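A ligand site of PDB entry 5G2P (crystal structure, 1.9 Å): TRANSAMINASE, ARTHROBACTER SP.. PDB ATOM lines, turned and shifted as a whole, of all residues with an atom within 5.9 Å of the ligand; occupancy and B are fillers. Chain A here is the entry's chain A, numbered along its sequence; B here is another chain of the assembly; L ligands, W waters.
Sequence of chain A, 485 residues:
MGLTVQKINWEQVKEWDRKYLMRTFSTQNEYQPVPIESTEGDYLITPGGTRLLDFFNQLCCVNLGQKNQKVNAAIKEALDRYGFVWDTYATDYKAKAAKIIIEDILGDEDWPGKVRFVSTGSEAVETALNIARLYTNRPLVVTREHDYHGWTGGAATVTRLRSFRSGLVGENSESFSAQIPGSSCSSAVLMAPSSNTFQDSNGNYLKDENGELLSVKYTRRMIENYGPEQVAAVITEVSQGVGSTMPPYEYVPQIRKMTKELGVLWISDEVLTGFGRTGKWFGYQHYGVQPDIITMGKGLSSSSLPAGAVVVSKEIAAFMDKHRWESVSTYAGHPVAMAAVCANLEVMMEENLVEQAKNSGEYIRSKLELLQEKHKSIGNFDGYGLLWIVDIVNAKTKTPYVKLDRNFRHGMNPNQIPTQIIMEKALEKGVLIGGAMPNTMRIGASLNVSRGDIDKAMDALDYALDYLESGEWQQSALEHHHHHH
C5 of the ligand is bonded to NZ of Lys 298 (1.5 Å).
OD2 of Asp 269 sits at hydrogen-bond distance from N1 of the ligand (2.7 Å).
The backbone NH of Thr 330 of chain B is in hydrogen-bond range of an oxygen (O5) of the ligand (2.9 Å).
The side-chain hydroxyl (OG1) of Thr 330 of chain B sits at hydrogen-bond distance from an oxygen (O5) of the ligand (2.7 Å).
An oxygen (O4) of the ligand lies within hydrogen-bond range of the backbone NH of Ser 122, at 2.9 Å.
The side-chain hydroxyl (OG) of Ser 122 lies within hydrogen-bond range of an oxygen (O4) of the ligand (2.8 Å).
The backbone NH (N) of Gly 121 is in hydrogen-bond range of an oxygen (O3) of the ligand (3.0 Å).
N of Lys 298 sits at hydrogen-bond distance from OH of Tyr 331 of chain B, 3.2 Å away.
The side-chain hydroxyl of Thr 295 is in hydrogen-bond range of the side-chain carboxylate of Asp 269.
OE2 of Glu 237 is in hydrogen-bond range of N of Tyr 148 (2.8 Å).
The side-chain carboxylate (OE1) of Glu 237 sits at hydrogen-bond distance from the backbone NH (N) of Gly 241, at 2.9 Å.
OH of Tyr 148 lies within hydrogen-bond range of O of Val 328 of chain B, 3.3 Å away.
The backbone carbonyl oxygen (O) of Thr 295 is in hydrogen-bond range of the backbone NH (N) of Val 271.
The side-chain carboxylate (OE2) of Glu 123 of chain B lies within hydrogen-bond range of the side-chain hydroxyl (OG1) of Thr 120 (2.9 Å).
The backbone NH of Glu 123 of chain A sits at hydrogen-bond distance from the side-chain hydroxyl of Thr 120 (3.1 Å).
Residues that only touch the ligand: Thr 120 (3.8 Å), Tyr 148 (3.3 Å), His 149 (3.4 Å), Gly 150 (3.7 Å), Trp 151 (3.98 Å), Glu 237 (3.2 Å), Val 271 (3.5 Å), Leu 272 (3.4 Å) and Ser 329 of chain B (3.8 Å).
Hydrophobic or aromatic side chains within 4 Å of the ligand: Tyr 148, Val 271 and Leu 272.
14 residues have an atom within 4 Å of the ligand: Thr 120, Gly 121, Ser 122, Tyr 148, His 149, Gly 150, Trp 151, Glu 237, Asp 269, Val 271, Leu 272, Lys 298, Ser 329 of chain B and Thr 330 of chain B.
Along chain A the residues within 4 Å of the ligand span positions 120 to 298.
The nearest printed residue that does not touch the ligand is Val 125 (4.3 Å).
Water W3 lies within hydrogen-bond range of an oxygen (O4) of the ligand, the side-chain carboxylate of Glu 123 of chain B, the side-chain hydroxyl of Ser 329 of chain B and the indole nitrogen of Trp 151.
Water W6 bridges O3 of the ligand (2.7 Å) and N of Lys 298 (2.9 Å).
Water W1 lies within hydrogen-bond range of the side-chain hydroxyl (OH) of Tyr 148 (2.6 Å), the backbone carbonyl oxygen (O) of Val 328 of chain B (2.7 Å) and an oxygen (O5) of the ligand (2.7 Å).
Water W5 lies within hydrogen-bond range of O3 of the ligand (2.7 Å) and N of Tyr 331 of chain B (2.8 Å).
Water W2 lies within hydrogen-bond range of the side-chain carboxylate (OE1) of Glu 237 (2.8 Å), an oxygen (O1) of the ligand (2.9 Å) and the backbone NH (N) of Val 242 (3.0 Å).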
ATOM      1  N   LEU A  59      18.591 -16.518  15.223  1.00  0.00           N
ATOM      2  CA  LEU A  59      18.728 -15.406  16.206  1.00  0.00           C
ATOM      3  C   LEU A  59      20.053 -15.574  16.997  1.00  0.00           C
ATOM      4  O   LEU A  59      20.065 -15.578  18.242  1.00  0.00           O
ATOM      5  CB  LEU A  59      17.515 -15.383  17.137  1.00  0.00           C
ATOM      6  CG  LEU A  59      16.169 -15.169  16.415  1.00  0.00           C
ATOM      7  CD1 LEU A  59      14.957 -15.578  17.241  1.00  0.00           C
ATOM      8  CD2 LEU A  59      16.033 -13.723  15.950  1.00  0.00           C
ATOM      9  N   THR A 120      13.302 -21.845  28.116  1.00  0.00           N
ATOM     10  CA  THR A 120      13.649 -20.720  27.221  1.00  0.00           C
ATOM     11  C   THR A 120      14.533 -19.718  27.919  1.00  0.00           C
ATOM     12  O   THR A 120      14.667 -19.730  29.148  1.00  0.00           O
ATOM     13  CB  THR A 120      12.396 -19.953  26.723  1.00  0.00           C
ATOM     14  OG1 THR A 120      11.767 -19.285  27.831  1.00  0.00           O
ATOM     15  CG2 THR A 120      11.376 -20.885  26.088  1.00  0.00           C
ATOM     16  N   GLY A 121      15.132 -18.816  27.138  1.00  0.00           N
ATOM     17  CA  GLY A 121      15.931 -17.708  27.718  1.00  0.00           C
ATOM     18  C   GLY A 121      15.150 -16.725  28.605  1.00  0.00           C
ATOM     19  O   GLY A 121      15.671 -16.248  29.641  1.00  0.00           O
ATOM     20  N   SER A 122      13.910 -16.407  28.211  1.00  0.00           N
ATOM     21  CA  SER A 122      13.067 -15.537  29.050  1.00  0.00           C
ATOM     22  C   SER A 122      12.784 -16.237  30.384  1.00  0.00           C
ATOM     23  O   SER A 122      12.899 -15.642  31.438  1.00  0.00           O
ATOM     24  CB  SER A 122      11.742 -15.186  28.351  1.00  0.00           C
ATOM     25  OG  SER A 122      11.996 -14.350  27.228  1.00  0.00           O
ATOM     26  N   GLU A 123      12.422 -17.522  30.342  1.00  0.00           N
ATOM     27  CA  GLU A 123      12.250 -18.258  31.601  1.00  0.00           C
ATOM     28  C   GLU A 123      13.525 -18.263  32.497  1.00  0.00           C
ATOM     29  O   GLU A 123      13.428 -18.251  33.742  1.00  0.00           O
ATOM     30  CB  GLU A 123      11.760 -19.688  31.320  1.00  0.00           C
ATOM     31  CG  GLU A 123      10.284 -19.736  30.872  1.00  0.00           C
ATOM     32  CD  GLU A 123       9.690 -21.155  30.887  1.00  0.00           C
ATOM     33  OE1 GLU A 123      10.447 -22.159  30.895  1.00  0.00           O
ATOM     34  OE2 GLU A 123       8.433 -21.238  30.863  1.00  0.00           O
ATOM     35  N   VAL A 125      15.876 -15.897  32.592  1.00  0.00           N
ATOM     36  CA  VAL A 125      15.954 -14.548  33.145  1.00  0.00           C
ATOM     37  C   VAL A 125      14.944 -14.407  34.294  1.00  0.00           C
ATOM     38  O   VAL A 125      15.325 -13.860  35.330  1.00  0.00           O
ATOM     39  CB  VAL A 125      15.757 -13.450  32.053  1.00  0.00           C
ATOM     40  CG1 VAL A 125      15.486 -12.063  32.659  1.00  0.00           C
ATOM     41  CG2 VAL A 125      16.994 -13.379  31.161  1.00  0.00           C
ATOM     42  N   TYR A 148      18.149  -6.109  26.035  1.00  0.00           N
ATOM     43  CA  TYR A 148      17.091  -7.068  25.756  1.00  0.00           C
ATOM     44  C   TYR A 148      17.314  -8.307  26.632  1.00  0.00           C
ATOM     45  O   TYR A 148      18.392  -8.940  26.566  1.00  0.00           O
ATOM     46  CB  TYR A 148      17.035  -7.440  24.249  1.00  0.00           C
ATOM     47  CG  TYR A 148      15.826  -8.303  23.991  1.00  0.00           C
ATOM     48  CD1 TYR A 148      14.561  -7.715  23.841  1.00  0.00           C
ATOM     49  CD2 TYR A 148      15.919  -9.715  23.951  1.00  0.00           C
ATOM     50  CE1 TYR A 148      13.440  -8.512  23.643  1.00  0.00           C
ATOM     51  CE2 TYR A 148      14.802 -10.498  23.783  1.00  0.00           C
ATOM     52  CZ  TYR A 148      13.559  -9.879  23.617  1.00  0.00           C
ATOM     53  OH  TYR A 148      12.430 -10.635  23.472  1.00  0.00           O
ATOM     54  N   HIS A 149      16.333  -8.648  27.463  1.00  0.00           N
ATOM     55  CA  HIS A 149      16.472  -9.811  28.353  1.00  0.00           C
ATOM     56  C   HIS A 149      15.295 -10.759  28.245  1.00  0.00           C
ATOM     57  O   HIS A 149      15.127 -11.636  29.118  1.00  0.00           O
ATOM     58  CB  HIS A 149      16.697  -9.391  29.837  1.00  0.00           C
ATOM     59  CG  HIS A 149      17.948  -8.595  30.073  1.00  0.00           C
ATOM     60  ND1 HIS A 149      19.224  -9.148  29.999  1.00  0.00           N
ATOM     61  CD2 HIS A 149      18.132  -7.293  30.405  1.00  0.00           C
ATOM     62  CE1 HIS A 149      20.124  -8.214  30.268  1.00  0.00           C
ATOM     63  NE2 HIS A 149      19.475  -7.075  30.520  1.00  0.00           N
ATOM     64  N   GLY A 150      14.450 -10.582  27.219  1.00  0.00           N
ATOM     65  CA  GLY A 150      13.329 -11.506  26.977  1.00  0.00           C
ATOM     66  C   GLY A 150      11.999 -10.771  26.942  1.00  0.00           C
ATOM     67  O   GLY A 150      11.981  -9.558  27.004  1.00  0.00           O
ATOM     68  N   TRP A 151      10.903 -11.518  26.834  1.00  0.00           N
ATOM     69  CA  TRP A 151       9.585 -10.932  26.501  1.00  0.00           C
ATOM     70  C   TRP A 151       8.481 -11.248  27.539  1.00  0.00           C
ATOM     71  O   TRP A 151       7.455 -10.552  27.568  1.00  0.00           O
ATOM     72  CB  TRP A 151       9.143 -11.413  25.093  1.00  0.00           C
ATOM     73  CG  TRP A 151       8.854 -12.897  25.090  1.00  0.00           C
ATOM     74  CD1 TRP A 151       9.762 -13.916  24.882  1.00  0.00           C
ATOM     75  CD2 TRP A 151       7.597 -13.527  25.357  1.00  0.00           C
ATOM     76  NE1 TRP A 151       9.149 -15.119  25.023  1.00  0.00           N
ATOM     77  CE2 TRP A 151       7.821 -14.924  25.285  1.00  0.00           C
ATOM     78  CE3 TRP A 151       6.308 -13.051  25.625  1.00  0.00           C
ATOM     79  CZ2 TRP A 151       6.787 -15.862  25.488  1.00  0.00           C
ATOM     80  CZ3 TRP A 151       5.283 -13.981  25.863  1.00  0.00           C
ATOM     81  CH2 TRP A 151       5.533 -15.375  25.776  1.00  0.00           C
ATOM     82  N   GLU A 237      23.929  -7.355  29.619  1.00  0.00           N
ATOM     83  CA  GLU A 237      24.453  -8.120  28.514  1.00  0.00           C
ATOM     84  C   GLU A 237      25.883  -7.651  28.340  1.00  0.00           C
ATOM     85  O   GLU A 237      26.144  -6.467  28.275  1.00  0.00           O
ATOM     86  CB  GLU A 237      23.660  -7.804  27.234  1.00  0.00           C
ATOM     87  CG  GLU A 237      22.206  -8.167  27.294  1.00  0.00           C
ATOM     88  CD  GLU A 237      21.513  -7.818  25.992  1.00  0.00           C
ATOM     89  OE1 GLU A 237      21.584  -8.629  25.042  1.00  0.00           O
ATOM     90  OE2 GLU A 237      20.908  -6.738  25.938  1.00  0.00           O
ATOM     91  N   GLY A 241      22.744  -7.629  22.586  1.00  0.00           N
ATOM     92  CA  GLY A 241      22.429  -8.515  21.435  1.00  0.00           C
ATOM     93  C   GLY A 241      21.458  -7.863  20.472  1.00  0.00           C
ATOM     94  O   GLY A 241      21.860  -7.354  19.406  1.00  0.00           O
ATOM     95  N   VAL A 242      20.191  -7.834  20.838  1.00  0.00           N
ATOM     96  CA  VAL A 242      19.176  -7.217  19.987  1.00  0.00           C
ATOM     97  C   VAL A 242      19.537  -5.729  19.820  1.00  0.00           C
ATOM     98  O   VAL A 242      19.489  -5.177  18.704  1.00  0.00           O
ATOM     99  CB  VAL A 242      17.743  -7.439  20.549  1.00  0.00           C
ATOM    100  CG1 VAL A 242      16.704  -6.697  19.706  1.00  0.00           C
ATOM    101  CG2 VAL A 242      17.415  -8.941  20.538  1.00  0.00           C
ATOM    102  N   ASP A 269      23.605 -11.868  31.629  1.00  0.00           N
ATOM    103  CA  ASP A 269      22.660 -12.553  30.763  1.00  0.00           C
ATOM    104  C   ASP A 269      23.448 -13.030  29.549  1.00  0.00           C
ATOM    105  O   ASP A 269      23.784 -12.226  28.667  1.00  0.00           O
ATOM    106  CB  ASP A 269      21.505 -11.605  30.346  1.00  0.00           C
ATOM    107  CG  ASP A 269      20.471 -12.279  29.491  1.00  0.00           C
ATOM    108  OD1 ASP A 269      20.678 -13.442  29.055  1.00  0.00           O
ATOM    109  OD2 ASP A 269      19.419 -11.643  29.217  1.00  0.00           O
ATOM    110  N   GLU A 270      23.728 -14.329  29.530  1.00  0.00           N
ATOM    111  CA  GLU A 270      24.547 -14.977  28.504  1.00  0.00           C
ATOM    112  C   GLU A 270      23.678 -15.794  27.564  1.00  0.00           C
ATOM    113  O   GLU A 270      24.179 -16.684  26.893  1.00  0.00           O
ATOM    114  CB  GLU A 270      25.634 -15.873  29.167  1.00  0.00           C
ATOM    115  CG  GLU A 270      26.648 -15.138  30.039  1.00  0.00           C
ATOM    116  CD  GLU A 270      27.843 -14.604  29.251  1.00  0.00           C
ATOM    117  OE1 GLU A 270      28.033 -15.013  28.076  1.00  0.00           O
ATOM    118  OE2 GLU A 270      28.616 -13.783  29.827  1.00  0.00           O
ATOM    119  N   VAL A 271      22.380 -15.467  27.479  1.00  0.00           N
ATOM    120  CA  VAL A 271      21.471 -16.212  26.601  1.00  0.00           C
ATOM    121  C   VAL A 271      22.010 -16.207  25.177  1.00  0.00           C
ATOM    122  O   VAL A 271      22.058 -17.247  24.508  1.00  0.00           O
ATOM    123  CB  VAL A 271      19.999 -15.695  26.714  1.00  0.00           C
ATOM    124  CG1 VAL A 271      19.143 -16.229  25.562  1.00  0.00           C
ATOM    125  CG2 VAL A 271      19.418 -16.159  28.052  1.00  0.00           C
ATOM    126  N   LEU A 272      22.461 -15.037  24.747  1.00  0.00           N
ATOM    127  CA  LEU A 272      23.009 -14.897  23.403  1.00  0.00           C
ATOM    128  C   LEU A 272      24.555 -15.065  23.328  1.00  0.00           C
ATOM    129  O   LEU A 272      25.078 -15.756  22.427  1.00  0.00           O
ATOM    130  CB  LEU A 272      22.535 -13.564  22.809  1.00  0.00           C
ATOM    131  CG  LEU A 272      22.844 -13.043  21.385  1.00  0.00           C
ATOM    132  CD1 LEU A 272      23.793 -11.870  21.397  1.00  0.00           C
ATOM    133  CD2 LEU A 272      23.340 -14.099  20.443  1.00  0.00           C
ATOM    134  N   THR A 295      22.477 -16.359  33.068  1.00  0.00           N
ATOM    135  CA  THR A 295      21.293 -16.896  32.381  1.00  0.00           C
ATOM    136  C   THR A 295      21.668 -17.401  30.990  1.00  0.00           C
ATOM    137  O   THR A 295      22.489 -16.775  30.302  1.00  0.00           O
ATOM    138  CB  THR A 295      20.157 -15.859  32.223  1.00  0.00           C
ATOM    139  OG1 THR A 295      20.661 -14.679  31.594  1.00  0.00           O
ATOM    140  CG2 THR A 295      19.613 -15.479  33.582  1.00  0.00           C
ATOM    141  N   GLY A 297      20.323 -19.698  27.234  1.00  0.00           N
ATOM    142  CA  GLY A 297      19.378 -20.238  26.244  1.00  0.00           C
ATOM    143  C   GLY A 297      20.167 -20.421  24.958  1.00  0.00           C
ATOM    144  O   GLY A 297      21.373 -20.715  25.014  1.00  0.00           O
ATOM    145  N   LYS A 298      19.494 -20.308  23.813  1.00  0.00           N
ATOM    146  CA  LYS A 298      20.144 -20.342  22.464  1.00  0.00           C
ATOM    147  C   LYS A 298      21.243 -21.397  22.290  1.00  0.00           C
ATOM    148  O   LYS A 298      20.924 -22.573  22.033  1.00  0.00           O
ATOM    149  CB  LYS A 298      20.599 -18.910  22.094  1.00  0.00           C
ATOM    150  CG  LYS A 298      19.452 -17.872  22.149  1.00  0.00           C
ATOM    151  CD  LYS A 298      19.849 -16.444  21.682  1.00  0.00           C
ATOM    152  CE  LYS A 298      18.578 -15.578  21.464  1.00  0.00           C
ATOM    153  NZ  LYS A 298      18.313 -14.533  22.490  1.00  0.00           N
ATOM    154  N   GLU B 123       4.376 -19.251  29.284  1.00  0.00           N
ATOM    155  CA  GLU B 123       4.489 -18.359  28.096  1.00  0.00           C
ATOM    156  C   GLU B 123       3.156 -18.136  27.340  1.00  0.00           C
ATOM    157  O   GLU B 123       2.893 -17.016  26.852  1.00  0.00           O
ATOM    158  CB  GLU B 123       5.560 -18.852  27.108  1.00  0.00           C
ATOM    159  CG  GLU B 123       6.966 -18.620  27.615  1.00  0.00           C
ATOM    160  CD  GLU B 123       8.054 -18.969  26.626  1.00  0.00           C
ATOM    161  OE1 GLU B 123       7.790 -19.718  25.645  1.00  0.00           O
ATOM    162  OE2 GLU B 123       9.191 -18.484  26.863  1.00  0.00           O
ATOM    163  N   VAL B 328       9.005 -11.150  20.057  1.00  0.00           N
ATOM    164  CA  VAL B 328       9.802 -12.311  19.600  1.00  0.00           C
ATOM    165  C   VAL B 328      10.115 -13.199  20.810  1.00  0.00           C
ATOM    166  O   VAL B 328      10.462 -12.707  21.893  1.00  0.00           O
ATOM    167  CB  VAL B 328      11.111 -11.900  18.855  1.00  0.00           C
ATOM    168  CG1 VAL B 328      11.999 -10.994  19.713  1.00  0.00           C
ATOM    169  CG2 VAL B 328      11.908 -13.126  18.425  1.00  0.00           C
ATOM    170  N   SER B 329       9.923 -14.504  20.598  1.00  0.00           N
ATOM    171  CA  SER B 329      10.341 -15.579  21.480  1.00  0.00           C
ATOM    172  C   SER B 329      11.190 -16.491  20.622  1.00  0.00           C
ATOM    173  O   SER B 329      10.708 -17.000  19.622  1.00  0.00           O
ATOM    174  CB  SER B 329       9.088 -16.334  21.940  1.00  0.00           C
ATOM    175  OG  SER B 329       9.388 -17.587  22.537  1.00  0.00           O
ATOM    176  N   THR B 330      12.447 -16.736  21.002  1.00  0.00           N
ATOM    177  CA  THR B 330      13.357 -17.506  20.175  1.00  0.00           C
ATOM    178  C   THR B 330      12.751 -18.831  19.711  1.00  0.00           C
ATOM    179  O   THR B 330      12.640 -19.067  18.505  1.00  0.00           O
ATOM    180  CB  THR B 330      14.692 -17.764  20.889  1.00  0.00           C
ATOM    181  OG1 THR B 330      15.298 -16.522  21.223  1.00  0.00           O
ATOM    182  CG2 THR B 330      15.654 -18.569  19.949  1.00  0.00           C
ATOM    183  N   TYR B 331      12.276 -19.644  20.653  1.00  0.00           N
ATOM    184  CA  TYR B 331      11.825 -20.990  20.320  1.00  0.00           C
ATOM    185  C   TYR B 331      10.350 -21.117  19.934  1.00  0.00           C
ATOM    186  O   TYR B 331       9.894 -22.222  19.642  1.00  0.00           O
ATOM    187  CB  TYR B 331      12.113 -21.922  21.498  1.00  0.00           C
ATOM    188  CG  TYR B 331      13.598 -22.053  21.716  1.00  0.00           C
ATOM    189  CD1 TYR B 331      14.472 -22.039  20.626  1.00  0.00           C
ATOM    190  CD2 TYR B 331      14.134 -22.198  22.996  1.00  0.00           C
ATOM    191  CE1 TYR B 331      15.837 -22.168  20.802  1.00  0.00           C
ATOM    192  CE2 TYR B 331      15.491 -22.328  23.177  1.00  0.00           C
ATOM    193  CZ  TYR B 331      16.333 -22.317  22.073  1.00  0.00           C
ATOM    194  OH  TYR B 331      17.676 -22.448  22.213  1.00  0.00           O
HETATM  195  N1  LIG L   1      18.256 -12.528  26.942  1.00  0.00           N
HETATM  196  C1  LIG L   1      19.043 -12.254  25.860  1.00  0.00           C
HETATM  197  C2  LIG L   1      20.345 -11.478  25.982  1.00  0.00           C
HETATM  198  C3  LIG L   1      18.603 -12.687  24.523  1.00  0.00           C
HETATM  199  O1  LIG L   1      19.367 -12.415  23.422  1.00  0.00           O
HETATM  200  C4  LIG L   1      17.334 -13.430  24.363  1.00  0.00           C
HETATM  201  C5  LIG L   1      17.010 -13.891  22.941  1.00  0.00           C
HETATM  202  C6  LIG L   1      16.561 -13.686  25.627  1.00  0.00           C
HETATM  203  C7  LIG L   1      17.097 -13.225  26.837  1.00  0.00           C
HETATM  204  C8  LIG L   1      15.229 -14.405  25.678  1.00  0.00           C
HETATM  205  O2  LIG L   1      15.351 -15.756  25.277  1.00  0.00           O
HETATM  206  P1  LIG L   1      14.087 -16.459  24.598  1.00  0.00           P
HETATM  207  O3  LIG L   1      14.606 -17.870  24.388  1.00  0.00           O
HETATM  208  O4  LIG L   1      12.891 -16.363  25.531  1.00  0.00           O
HETATM  209  O5  LIG L   1      13.786 -15.690  23.327  1.00  0.00           O
HETATM  210  O   HOH W   1      12.727 -13.175  23.326  1.00  0.00           O
HETATM  211  O   HOH W   2      19.695  -9.513  23.218  1.00  0.00           O
HETATM  212  O   HOH W   3      10.649 -17.540  24.916  1.00  0.00           O
HETATM  213  O   HOH W   4      23.596 -12.660  26.033  1.00  0.00           O
HETATM  214  O   HOH W   5      12.504 -19.380  23.471  1.00  0.00           O
HETATM  215  O   HOH W   6      16.763 -19.440  23.890  1.00  0.00           O
